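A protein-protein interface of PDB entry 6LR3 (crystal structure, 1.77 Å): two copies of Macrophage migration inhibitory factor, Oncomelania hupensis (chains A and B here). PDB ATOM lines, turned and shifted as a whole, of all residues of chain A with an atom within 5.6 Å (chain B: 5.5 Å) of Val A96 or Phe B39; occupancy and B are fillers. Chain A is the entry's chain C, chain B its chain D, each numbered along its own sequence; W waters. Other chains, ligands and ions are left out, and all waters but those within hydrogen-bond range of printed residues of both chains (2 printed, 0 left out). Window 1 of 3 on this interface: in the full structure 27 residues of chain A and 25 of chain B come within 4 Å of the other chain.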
ATOM      1  N   ILE A  48      18.144 -27.652 -21.993  1.00  0.00           N
ATOM      2  CA  ILE A  48      19.590 -27.674 -22.251  1.00  0.00           C
ATOM      3  C   ILE A  48      19.797 -28.306 -23.623  1.00  0.00           C
ATOM      4  O   ILE A  48      19.261 -29.395 -23.897  1.00  0.00           O
ATOM      5  CB  ILE A  48      20.365 -28.372 -21.118  1.00  0.00           C
ATOM      6  CG1 ILE A  48      21.863 -28.308 -21.386  1.00  0.00           C
ATOM      7  CG2 ILE A  48      19.897 -29.815 -20.866  1.00  0.00           C
ATOM      8  CD1 ILE A  48      22.668 -28.701 -20.149  1.00  0.00           C
ATOM      9  N   MET A  49      20.438 -27.537 -24.491  1.00  0.00           N
ATOM     10  CA  MET A  49      20.819 -28.021 -25.823  1.00  0.00           C
ATOM     11  C   MET A  49      22.332 -28.130 -25.871  1.00  0.00           C
ATOM     12  O   MET A  49      23.042 -27.441 -25.102  1.00  0.00           O
ATOM     13  CB  MET A  49      20.223 -27.187 -26.952  1.00  0.00           C
ATOM     14  CG  MET A  49      20.833 -25.881 -27.173  1.00  0.00           C
ATOM     15  SD  MET A  49      20.512 -25.174 -28.893  1.00  0.00           S
ATOM     16  CE  MET A  49      18.743 -25.380 -29.030  1.00  0.00           C
ATOM     17  N   MET A  50      22.805 -29.038 -26.711  1.00  0.00           N
ATOM     18  CA  MET A  50      24.237 -29.290 -26.885  1.00  0.00           C
ATOM     19  C   MET A  50      24.487 -29.381 -28.385  1.00  0.00           C
ATOM     20  O   MET A  50      23.720 -30.079 -29.067  1.00  0.00           O
ATOM     21  CB  MET A  50      24.609 -30.602 -26.193  1.00  0.00           C
ATOM     22  CG  MET A  50      26.071 -30.925 -26.280  1.00  0.00           C
ATOM     23  SD  MET A  50      26.323 -32.604 -25.676  1.00  0.00           S
ATOM     24  CE  MET A  50      28.111 -32.662 -25.677  1.00  0.00           C
ATOM     25  N   GLY A  51      25.500 -28.686 -28.869  1.00  0.00           N
ATOM     26  CA  GLY A  51      25.861 -28.744 -30.302  1.00  0.00           C
ATOM     27  C   GLY A  51      24.789 -28.132 -31.165  1.00  0.00           C
ATOM     28  O   GLY A  51      24.718 -28.476 -32.357  1.00  0.00           O
ATOM     29  N   CYS A  57      21.182 -35.187 -23.957  1.00  0.00           N
ATOM     30  CA  CYS A  57      22.499 -34.769 -23.478  1.00  0.00           C
ATOM     31  C   CYS A  57      22.466 -34.619 -21.959  1.00  0.00           C
ATOM     32  O   CYS A  57      21.398 -34.562 -21.360  1.00  0.00           O
ATOM     33  CB  CYS A  57      22.950 -33.471 -24.150  1.00  0.00           C
ATOM     34  SG  CYS A  57      22.015 -32.012 -23.650  1.00  0.00           S
ATOM     35  N   VAL A  58      23.646 -34.581 -21.380  1.00  0.00           N
ATOM     36  CA  VAL A  58      23.841 -34.338 -19.918  1.00  0.00           C
ATOM     37  C   VAL A  58      25.024 -33.410 -19.747  1.00  0.00           C
ATOM     38  O   VAL A  58      26.089 -33.690 -20.289  1.00  0.00           O
ATOM     39  CB  VAL A  58      24.137 -35.636 -19.142  1.00  0.00           C
ATOM     40  CG1 VAL A  58      24.402 -35.312 -17.680  1.00  0.00           C
ATOM     41  CG2 VAL A  58      23.040 -36.667 -19.312  1.00  0.00           C
ATOM     42  N   PHE A  59      24.839 -32.387 -18.931  1.00  0.00           N
ATOM     43  CA  PHE A  59      25.941 -31.661 -18.284  1.00  0.00           C
ATOM     44  C   PHE A  59      25.771 -31.878 -16.798  1.00  0.00           C
ATOM     45  O   PHE A  59      24.742 -31.488 -16.234  1.00  0.00           O
ATOM     46  CB  PHE A  59      25.936 -30.174 -18.631  1.00  0.00           C
ATOM     47  CG  PHE A  59      26.973 -29.423 -17.846  1.00  0.00           C
ATOM     48  CD1 PHE A  59      28.296 -29.793 -17.928  1.00  0.00           C
ATOM     49  CD2 PHE A  59      26.634 -28.359 -17.024  1.00  0.00           C
ATOM     50  CE1 PHE A  59      29.268 -29.142 -17.191  1.00  0.00           C
ATOM     51  CE2 PHE A  59      27.604 -27.694 -16.293  1.00  0.00           C
ATOM     52  CZ  PHE A  59      28.928 -28.089 -16.384  1.00  0.00           C
ATOM     53  N   ALA A  60      26.759 -32.505 -16.169  1.00  0.00           N
ATOM     54  CA  ALA A  60      26.687 -32.793 -14.730  1.00  0.00           C
ATOM     55  C   ALA A  60      27.864 -32.119 -14.028  1.00  0.00           C
ATOM     56  O   ALA A  60      28.908 -31.908 -14.680  1.00  0.00           O
ATOM     57  CB  ALA A  60      26.666 -34.273 -14.479  1.00  0.00           C
ATOM     58  N   ARG A  94      27.502 -37.377 -25.684  1.00  0.00           N
ATOM     59  CA  ARG A  94      26.559 -36.298 -25.341  1.00  0.00           C
ATOM     60  C   ARG A  94      26.635 -36.015 -23.838  1.00  0.00           C
ATOM     61  O   ARG A  94      25.662 -35.452 -23.276  1.00  0.00           O
ATOM     62  CB  ARG A  94      25.153 -36.655 -25.799  1.00  0.00           C
ATOM     63  CG  ARG A  94      25.021 -36.737 -27.309  1.00  0.00           C
ATOM     64  CD  ARG A  94      25.019 -35.378 -27.965  1.00  0.00           C
ATOM     65  NE  ARG A  94      23.765 -34.678 -27.706  1.00  0.00           N
ATOM     66  CZ  ARG A  94      23.472 -33.488 -28.213  1.00  0.00           C
ATOM     67  NH1 ARG A  94      24.335 -32.868 -28.988  1.00  0.00           N
ATOM     68  NH2 ARG A  94      22.329 -32.900 -27.921  1.00  0.00           N
ATOM     69  N   ILE A  95      27.736 -36.400 -23.199  1.00  0.00           N
ATOM     70  CA  ILE A  95      27.904 -36.215 -21.723  1.00  0.00           C
ATOM     71  C   ILE A  95      29.165 -35.401 -21.455  1.00  0.00           C
ATOM     72  O   ILE A  95      30.230 -35.797 -21.897  1.00  0.00           O
ATOM     73  CB  ILE A  95      27.967 -37.563 -20.985  1.00  0.00           C
ATOM     74  CG1 ILE A  95      26.735 -38.410 -21.274  1.00  0.00           C
ATOM     75  CG2 ILE A  95      28.175 -37.355 -19.499  1.00  0.00           C
ATOM     76  CD1 ILE A  95      26.878 -39.866 -20.856  1.00  0.00           C
ATOM     77  N   VAL A  96      29.004 -34.354 -20.656  1.00  0.00           N
ATOM     78  CA  VAL A  96      30.132 -33.557 -20.124  1.00  0.00           C
ATOM     79  C   VAL A  96      29.941 -33.469 -18.612  1.00  0.00           C
ATOM     80  O   VAL A  96      28.829 -33.238 -18.156  1.00  0.00           O
ATOM     81  CB  VAL A  96      30.205 -32.178 -20.779  1.00  0.00           C
ATOM     82  CG1 VAL A  96      31.167 -31.251 -20.052  1.00  0.00           C
ATOM     83  CG2 VAL A  96      30.594 -32.309 -22.242  1.00  0.00           C
ATOM     84  N   ILE A  97      30.999 -33.655 -17.864  1.00  0.00           N
ATOM     85  CA  ILE A  97      30.974 -33.600 -16.378  1.00  0.00           C
ATOM     86  C   ILE A  97      32.085 -32.665 -15.914  1.00  0.00           C
ATOM     87  O   ILE A  97      33.218 -32.826 -16.333  1.00  0.00           O
ATOM     88  CB  ILE A  97      31.110 -34.998 -15.748  1.00  0.00           C
ATOM     89  CG1 ILE A  97      30.098 -35.995 -16.310  1.00  0.00           C
ATOM     90  CG2 ILE A  97      31.032 -34.870 -14.238  1.00  0.00           C
ATOM     91  CD1 ILE A  97      30.436 -37.449 -16.043  1.00  0.00           C
ATOM     92  N   ARG A  98      31.746 -31.714 -15.063  1.00  0.00           N
ATOM     93  CA  ARG A  98      32.724 -30.806 -14.451  1.00  0.00           C
ATOM     94  C   ARG A  98      32.875 -31.197 -12.985  1.00  0.00           C
ATOM     95  O   ARG A  98      31.889 -31.340 -12.263  1.00  0.00           O
ATOM     96  CB  ARG A  98      32.288 -29.358 -14.583  1.00  0.00           C
ATOM     97  CG  ARG A  98      33.221 -28.372 -13.917  1.00  0.00           C
ATOM     98  CD  ARG A  98      32.749 -26.959 -14.123  1.00  0.00           C
ATOM     99  NE  ARG A  98      33.491 -26.149 -13.189  1.00  0.00           N
ATOM    100  CZ  ARG A  98      33.033 -25.118 -12.521  1.00  0.00           C
ATOM    101  NH1 ARG A  98      31.825 -24.637 -12.742  1.00  0.00           N
ATOM    102  NH2 ARG A  98      33.808 -24.559 -11.600  1.00  0.00           N
ATOM    103  N   PRO B   2      32.020 -25.981 -23.842  1.00  0.00           N
ATOM    104  CA  PRO B   2      31.654 -24.898 -22.880  1.00  0.00           C
ATOM    105  C   PRO B   2      30.181 -25.005 -22.493  1.00  0.00           C
ATOM    106  O   PRO B   2      29.404 -25.641 -23.199  1.00  0.00           O
ATOM    107  CB  PRO B   2      31.862 -23.541 -23.575  1.00  0.00           C
ATOM    108  CG  PRO B   2      32.834 -23.873 -24.683  1.00  0.00           C
ATOM    109  CD  PRO B   2      32.448 -25.291 -25.085  1.00  0.00           C
ATOM    110  N   VAL B   3      29.820 -24.362 -21.389  1.00  0.00           N
ATOM    111  CA  VAL B   3      28.406 -24.346 -20.954  1.00  0.00           C
ATOM    112  C   VAL B   3      28.023 -22.883 -20.749  1.00  0.00           C
ATOM    113  O   VAL B   3      28.663 -22.192 -19.921  1.00  0.00           O
ATOM    114  CB  VAL B   3      28.178 -25.166 -19.677  1.00  0.00           C
ATOM    115  CG1 VAL B   3      26.715 -25.098 -19.289  1.00  0.00           C
ATOM    116  CG2 VAL B   3      28.609 -26.617 -19.854  1.00  0.00           C
ATOM    117  N   ILE B   4      27.000 -22.443 -21.451  1.00  0.00           N
ATOM    118  CA  ILE B   4      26.382 -21.117 -21.223  1.00  0.00           C
ATOM    119  C   ILE B   4      25.084 -21.388 -20.471  1.00  0.00           C
ATOM    120  O   ILE B   4      24.193 -22.036 -21.042  1.00  0.00           O
ATOM    121  CB  ILE B   4      26.096 -20.381 -22.545  1.00  0.00           C
ATOM    122  CG1 ILE B   4      27.224 -20.502 -23.579  1.00  0.00           C
ATOM    123  CG2 ILE B   4      25.710 -18.950 -22.257  1.00  0.00           C
ATOM    124  CD1 ILE B   4      28.560 -20.119 -23.104  1.00  0.00           C
ATOM    125  N   THR B   5      24.967 -20.872 -19.270  1.00  0.00           N
ATOM    126  CA  THR B   5      23.790 -21.054 -18.420  1.00  0.00           C
ATOM    127  C   THR B   5      23.137 -19.685 -18.290  1.00  0.00           C
ATOM    128  O   THR B   5      23.821 -18.707 -17.946  1.00  0.00           O
ATOM    129  CB  THR B   5      24.142 -21.626 -17.049  1.00  0.00           C
ATOM    130  OG1 THR B   5      24.812 -22.851 -17.285  1.00  0.00           O
ATOM    131  CG2 THR B   5      22.931 -21.878 -16.197  1.00  0.00           C
ATOM    132  N   THR B  24      24.307 -20.309 -29.076  1.00  0.00           N
ATOM    133  CA  THR B  24      25.256 -21.399 -29.355  1.00  0.00           C
ATOM    134  C   THR B  24      26.224 -20.941 -30.437  1.00  0.00           C
ATOM    135  O   THR B  24      27.429 -21.044 -30.244  1.00  0.00           O
ATOM    136  CB  THR B  24      24.538 -22.681 -29.797  1.00  0.00           C
ATOM    137  OG1 THR B  24      23.741 -23.159 -28.705  1.00  0.00           O
ATOM    138  CG2 THR B  24      25.507 -23.740 -30.276  1.00  0.00           C
ATOM    139  N   VAL B  37      30.354 -29.437 -28.485  1.00  0.00           N
ATOM    140  CA  VAL B  37      30.452 -29.482 -26.999  1.00  0.00           C
ATOM    141  C   VAL B  37      29.984 -28.144 -26.407  1.00  0.00           C
ATOM    142  O   VAL B  37      30.267 -27.884 -25.239  1.00  0.00           O
ATOM    143  CB  VAL B  37      31.862 -29.856 -26.529  1.00  0.00           C
ATOM    144  CG1 VAL B  37      32.191 -31.257 -26.977  1.00  0.00           C
ATOM    145  CG2 VAL B  37      32.924 -28.895 -27.039  1.00  0.00           C
ATOM    146  N   MET B  38      29.244 -27.353 -27.170  1.00  0.00           N
ATOM    147  CA  MET B  38      28.662 -26.091 -26.656  1.00  0.00           C
ATOM    148  C   MET B  38      27.261 -26.388 -26.111  1.00  0.00           C
ATOM    149  O   MET B  38      26.362 -26.804 -26.879  1.00  0.00           O
ATOM    150  CB  MET B  38      28.539 -25.048 -27.774  1.00  0.00           C
ATOM    151  CG  MET B  38      27.917 -23.727 -27.290  1.00  0.00           C
ATOM    152  SD  MET B  38      29.036 -22.835 -26.118  1.00  0.00           S
ATOM    153  CE  MET B  38      30.507 -22.746 -27.144  1.00  0.00           C
ATOM    154  N   PHE B  39      27.060 -26.188 -24.814  1.00  0.00           N
ATOM    155  CA  PHE B  39      25.737 -26.302 -24.211  1.00  0.00           C
ATOM    156  C   PHE B  39      25.207 -24.891 -23.981  1.00  0.00           C
ATOM    157  O   PHE B  39      25.955 -23.999 -23.558  1.00  0.00           O
ATOM    158  CB  PHE B  39      25.778 -26.981 -22.849  1.00  0.00           C
ATOM    159  CG  PHE B  39      26.174 -28.424 -22.849  1.00  0.00           C
ATOM    160  CD1 PHE B  39      27.514 -28.776 -22.876  1.00  0.00           C
ATOM    161  CD2 PHE B  39      25.227 -29.412 -22.665  1.00  0.00           C
ATOM    162  CE1 PHE B  39      27.891 -30.104 -22.748  1.00  0.00           C
ATOM    163  CE2 PHE B  39      25.613 -30.734 -22.517  1.00  0.00           C
ATOM    164  CZ  PHE B  39      26.934 -31.073 -22.595  1.00  0.00           C
ATOM    165  N   VAL B  40      23.903 -24.744 -24.197  1.00  0.00           N
ATOM    166  CA  VAL B  40      23.164 -23.583 -23.668  1.00  0.00           C
ATOM    167  C   VAL B  40      22.021 -24.150 -22.833  1.00  0.00           C
ATOM    168  O   VAL B  40      21.140 -24.828 -23.371  1.00  0.00           O
ATOM    169  CB  VAL B  40      22.676 -22.627 -24.768  1.00  0.00           C
ATOM    170  CG1 VAL B  40      21.872 -21.503 -24.151  1.00  0.00           C
ATOM    171  CG2 VAL B  40      23.827 -22.117 -25.604  1.00  0.00           C
ATOM    172  N   ASP B  41      22.095 -23.880 -21.545  1.00  0.00           N
ATOM    173  CA  ASP B  41      21.138 -24.339 -20.519  1.00  0.00           C
ATOM    174  C   ASP B  41      20.330 -23.098 -20.147  1.00  0.00           C
ATOM    175  O   ASP B  41      20.851 -22.218 -19.435  1.00  0.00           O
ATOM    176  CB  ASP B  41      21.900 -24.977 -19.363  1.00  0.00           C
ATOM    177  CG  ASP B  41      21.040 -25.564 -18.273  1.00  0.00           C
ATOM    178  OD1 ASP B  41      19.822 -25.392 -18.371  1.00  0.00           O
ATOM    179  OD2 ASP B  41      21.619 -26.171 -17.346  1.00  0.00           O
ATOM    180  N   CYS B 107      37.264 -31.726 -16.124  1.00  0.00           N
ATOM    181  CA  CYS B 107      36.080 -31.752 -16.996  1.00  0.00           C
ATOM    182  C   CYS B 107      36.197 -32.909 -17.980  1.00  0.00           C
ATOM    183  O   CYS B 107      37.242 -33.039 -18.627  1.00  0.00           O
ATOM    184  CB  CYS B 107      35.935 -30.412 -17.673  1.00  0.00           C
ATOM    185  SG  CYS B 107      34.392 -30.321 -18.595  1.00  0.00           S
ATOM    186  N   SER B 108      35.198 -33.761 -18.032  1.00  0.00           N
ATOM    187  CA  SER B 108      35.174 -34.920 -18.952  1.00  0.00           C
ATOM    188  C   SER B 108      34.259 -34.620 -20.123  1.00  0.00           C
ATOM    189  O   SER B 108      33.258 -33.879 -19.976  1.00  0.00           O
ATOM    190  CB  SER B 108      34.761 -36.177 -18.267  1.00  0.00           C
ATOM    191  OG  SER B 108      33.439 -36.040 -17.767  1.00  0.00           O
ATOM    192  N   PHE B 109      34.561 -35.245 -21.250  1.00  0.00           N
ATOM    193  CA  PHE B 109      33.673 -35.339 -22.416  1.00  0.00           C
ATOM    194  C   PHE B 109      33.915 -36.709 -23.050  1.00  0.00           C
ATOM    195  O   PHE B 109      35.078 -37.016 -23.341  1.00  0.00           O
ATOM    196  CB  PHE B 109      33.954 -34.206 -23.408  1.00  0.00           C
ATOM    197  CG  PHE B 109      33.287 -34.437 -24.743  1.00  0.00           C
ATOM    198  CD1 PHE B 109      31.916 -34.620 -24.835  1.00  0.00           C
ATOM    199  CD2 PHE B 109      34.043 -34.546 -25.910  1.00  0.00           C
ATOM    200  CE1 PHE B 109      31.309 -34.818 -26.069  1.00  0.00           C
ATOM    201  CE2 PHE B 109      33.432 -34.766 -27.130  1.00  0.00           C
ATOM    202  CZ  PHE B 109      32.061 -34.894 -27.217  1.00  0.00           C
ATOM    203  N   HIS B 114      39.801 -33.471 -20.733  1.00  0.00           N
ATOM    204  CA  HIS B 114      40.227 -32.609 -21.847  1.00  0.00           C
ATOM    205  C   HIS B 114      41.742 -32.516 -21.950  1.00  0.00           C
ATOM    206  O   HIS B 114      42.453 -32.528 -20.891  1.00  0.00           O
ATOM    207  CB  HIS B 114      39.622 -31.244 -21.690  1.00  0.00           C
ATOM    208  CG  HIS B 114      38.167 -31.279 -21.984  1.00  0.00           C
ATOM    209  ND1 HIS B 114      37.265 -31.781 -21.079  1.00  0.00           N
ATOM    210  CD2 HIS B 114      37.460 -30.927 -23.083  1.00  0.00           C
ATOM    211  CE1 HIS B 114      36.054 -31.698 -21.597  1.00  0.00           C
ATOM    212  NE2 HIS B 114      36.137 -31.169 -22.800  1.00  0.00           N
HETATM  213  O   HOH W   1      23.974 -25.890 -28.064  1.00  0.00           O
HETATM  214  O   HOH W   2      31.784 -36.906 -19.620  1.00  0.00           O
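O of Ile B4 lies within hydrogen-bond range of N of Asp B41, at 2.8 Å. A ring nitrogen (ND1) of His B114 is in hydrogen-bond range of the backbone carbonyl oxygen of Cys B107 (2.8 Å). The backbone NH of Val A58 is in hydrogen-bond range of the backbone carbonyl oxygen of Arg A94 (2.9 Å). N of Ile B4 lies within hydrogen-bond range of O of Phe B39 (2.8 Å). The backbone carbonyl oxygen (O) of Val A96 lies within hydrogen-bond range of the backbone NH (N) of Ala A60, at 3.0 Å. The backbone carbonyl oxygen of Met A50 sits at hydrogen-bond distance from the guanidinium group of Arg A94 (2.9 Å).
The backbone NH (N) of Ser B108 is in hydrogen-bond range of the backbone carbonyl oxygen (O) of Ile A97, 2.8 Å away. The backbone carbonyl oxygen (O) of Ile A97 lies close to the side-chain sulfur (SG) of Cys B107. The backbone NH (N) of Gly A51 sits at hydrogen-bond distance from the backbone carbonyl oxygen (O) of Met B38. The backbone NH of Val B40 sits at hydrogen-bond distance from the backbone carbonyl oxygen of Met A49 (3.0 Å).
Water W2 bridges the side-chain hydroxyl of Ser B108 and the backbone carbonyl oxygen of Ile A95. Water W1 lies within hydrogen-bond range of the side-chain hydroxyl of Thr B24, the backbone carbonyl oxygen of Met B38, the backbone NH of Gly A51 and the backbone carbonyl oxygen of Met A49.
No position is printed for both chains. Of the 22 pairs that touch across the chains among the printed residues, none has its exchanged pair printed and touching as well.
CD1 of Ile A48 touches CB of Asp B41, at 3.9 Å. Met A49 touches Thr B24 (SD to OG1, 3.8 Å). Met A50 touches Phe B109 (CE to CE1, 3.9 Å). Phe B39 touches Cys A57. Phe B39 touches Val A58 (CZ to O, 3.6 Å). Phe A59 touches Val B3. Ile A95 touches Phe B109. Phe B39 touches Val A96. Cys B107 touches Val A96. Phe B109 touches Val A96.
Of the 13 printed residues of chain A, 10 touch a printed residue of chain B. Printed residues of chain B that touch a printed residue of chain A: Val B3, Thr B24, Met B38, Phe B39, Val B40, Asp B41, Cys B107, Ser B108 and Phe B109. Hydrophobic or aromatic side chains of chain B within 4 Å of the printed part of chain A: Val B3, Phe B39 and Phe B109. Among the printed residues, 22 pairs touch across the chains.
Of the printed residues of chain B, Ile A48 touches Phe B39, Val B40 and Asp B41. Printed residues of chain B within 4 Å of Phe A59: Val B3 (3.7 Å) and Phe B39 (3.9 Å). Arg A94 touches none of the printed residues of chain B. Of the printed residues of chain B, Ile A95 touches Phe B109. Val A96 touches just these residues of chain B: Phe B39 (3.5 Å), Cys B107 (3.7 Å), Ser B108 (3.1 Å) and Phe B109 (3.7 Å). Pro B2 touches none of the printed residues of chain A. Printed residues of chain A within 4 Å of Thr B24: Met A49 (3.8 Å). Printed residues of chain A within 4 Å of Asp B41: Ile A48 (3.9 Å). The nearest residue of chain B that does not touch Val A96 is Val B37 (5.1 Å). The nearest printed residue of chain A that does not touch Phe B39 is Arg A94 (4.6 Å). The nearest printed residue of chain B that does not touch Cys A57 is Val B40 (7.2 Å).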
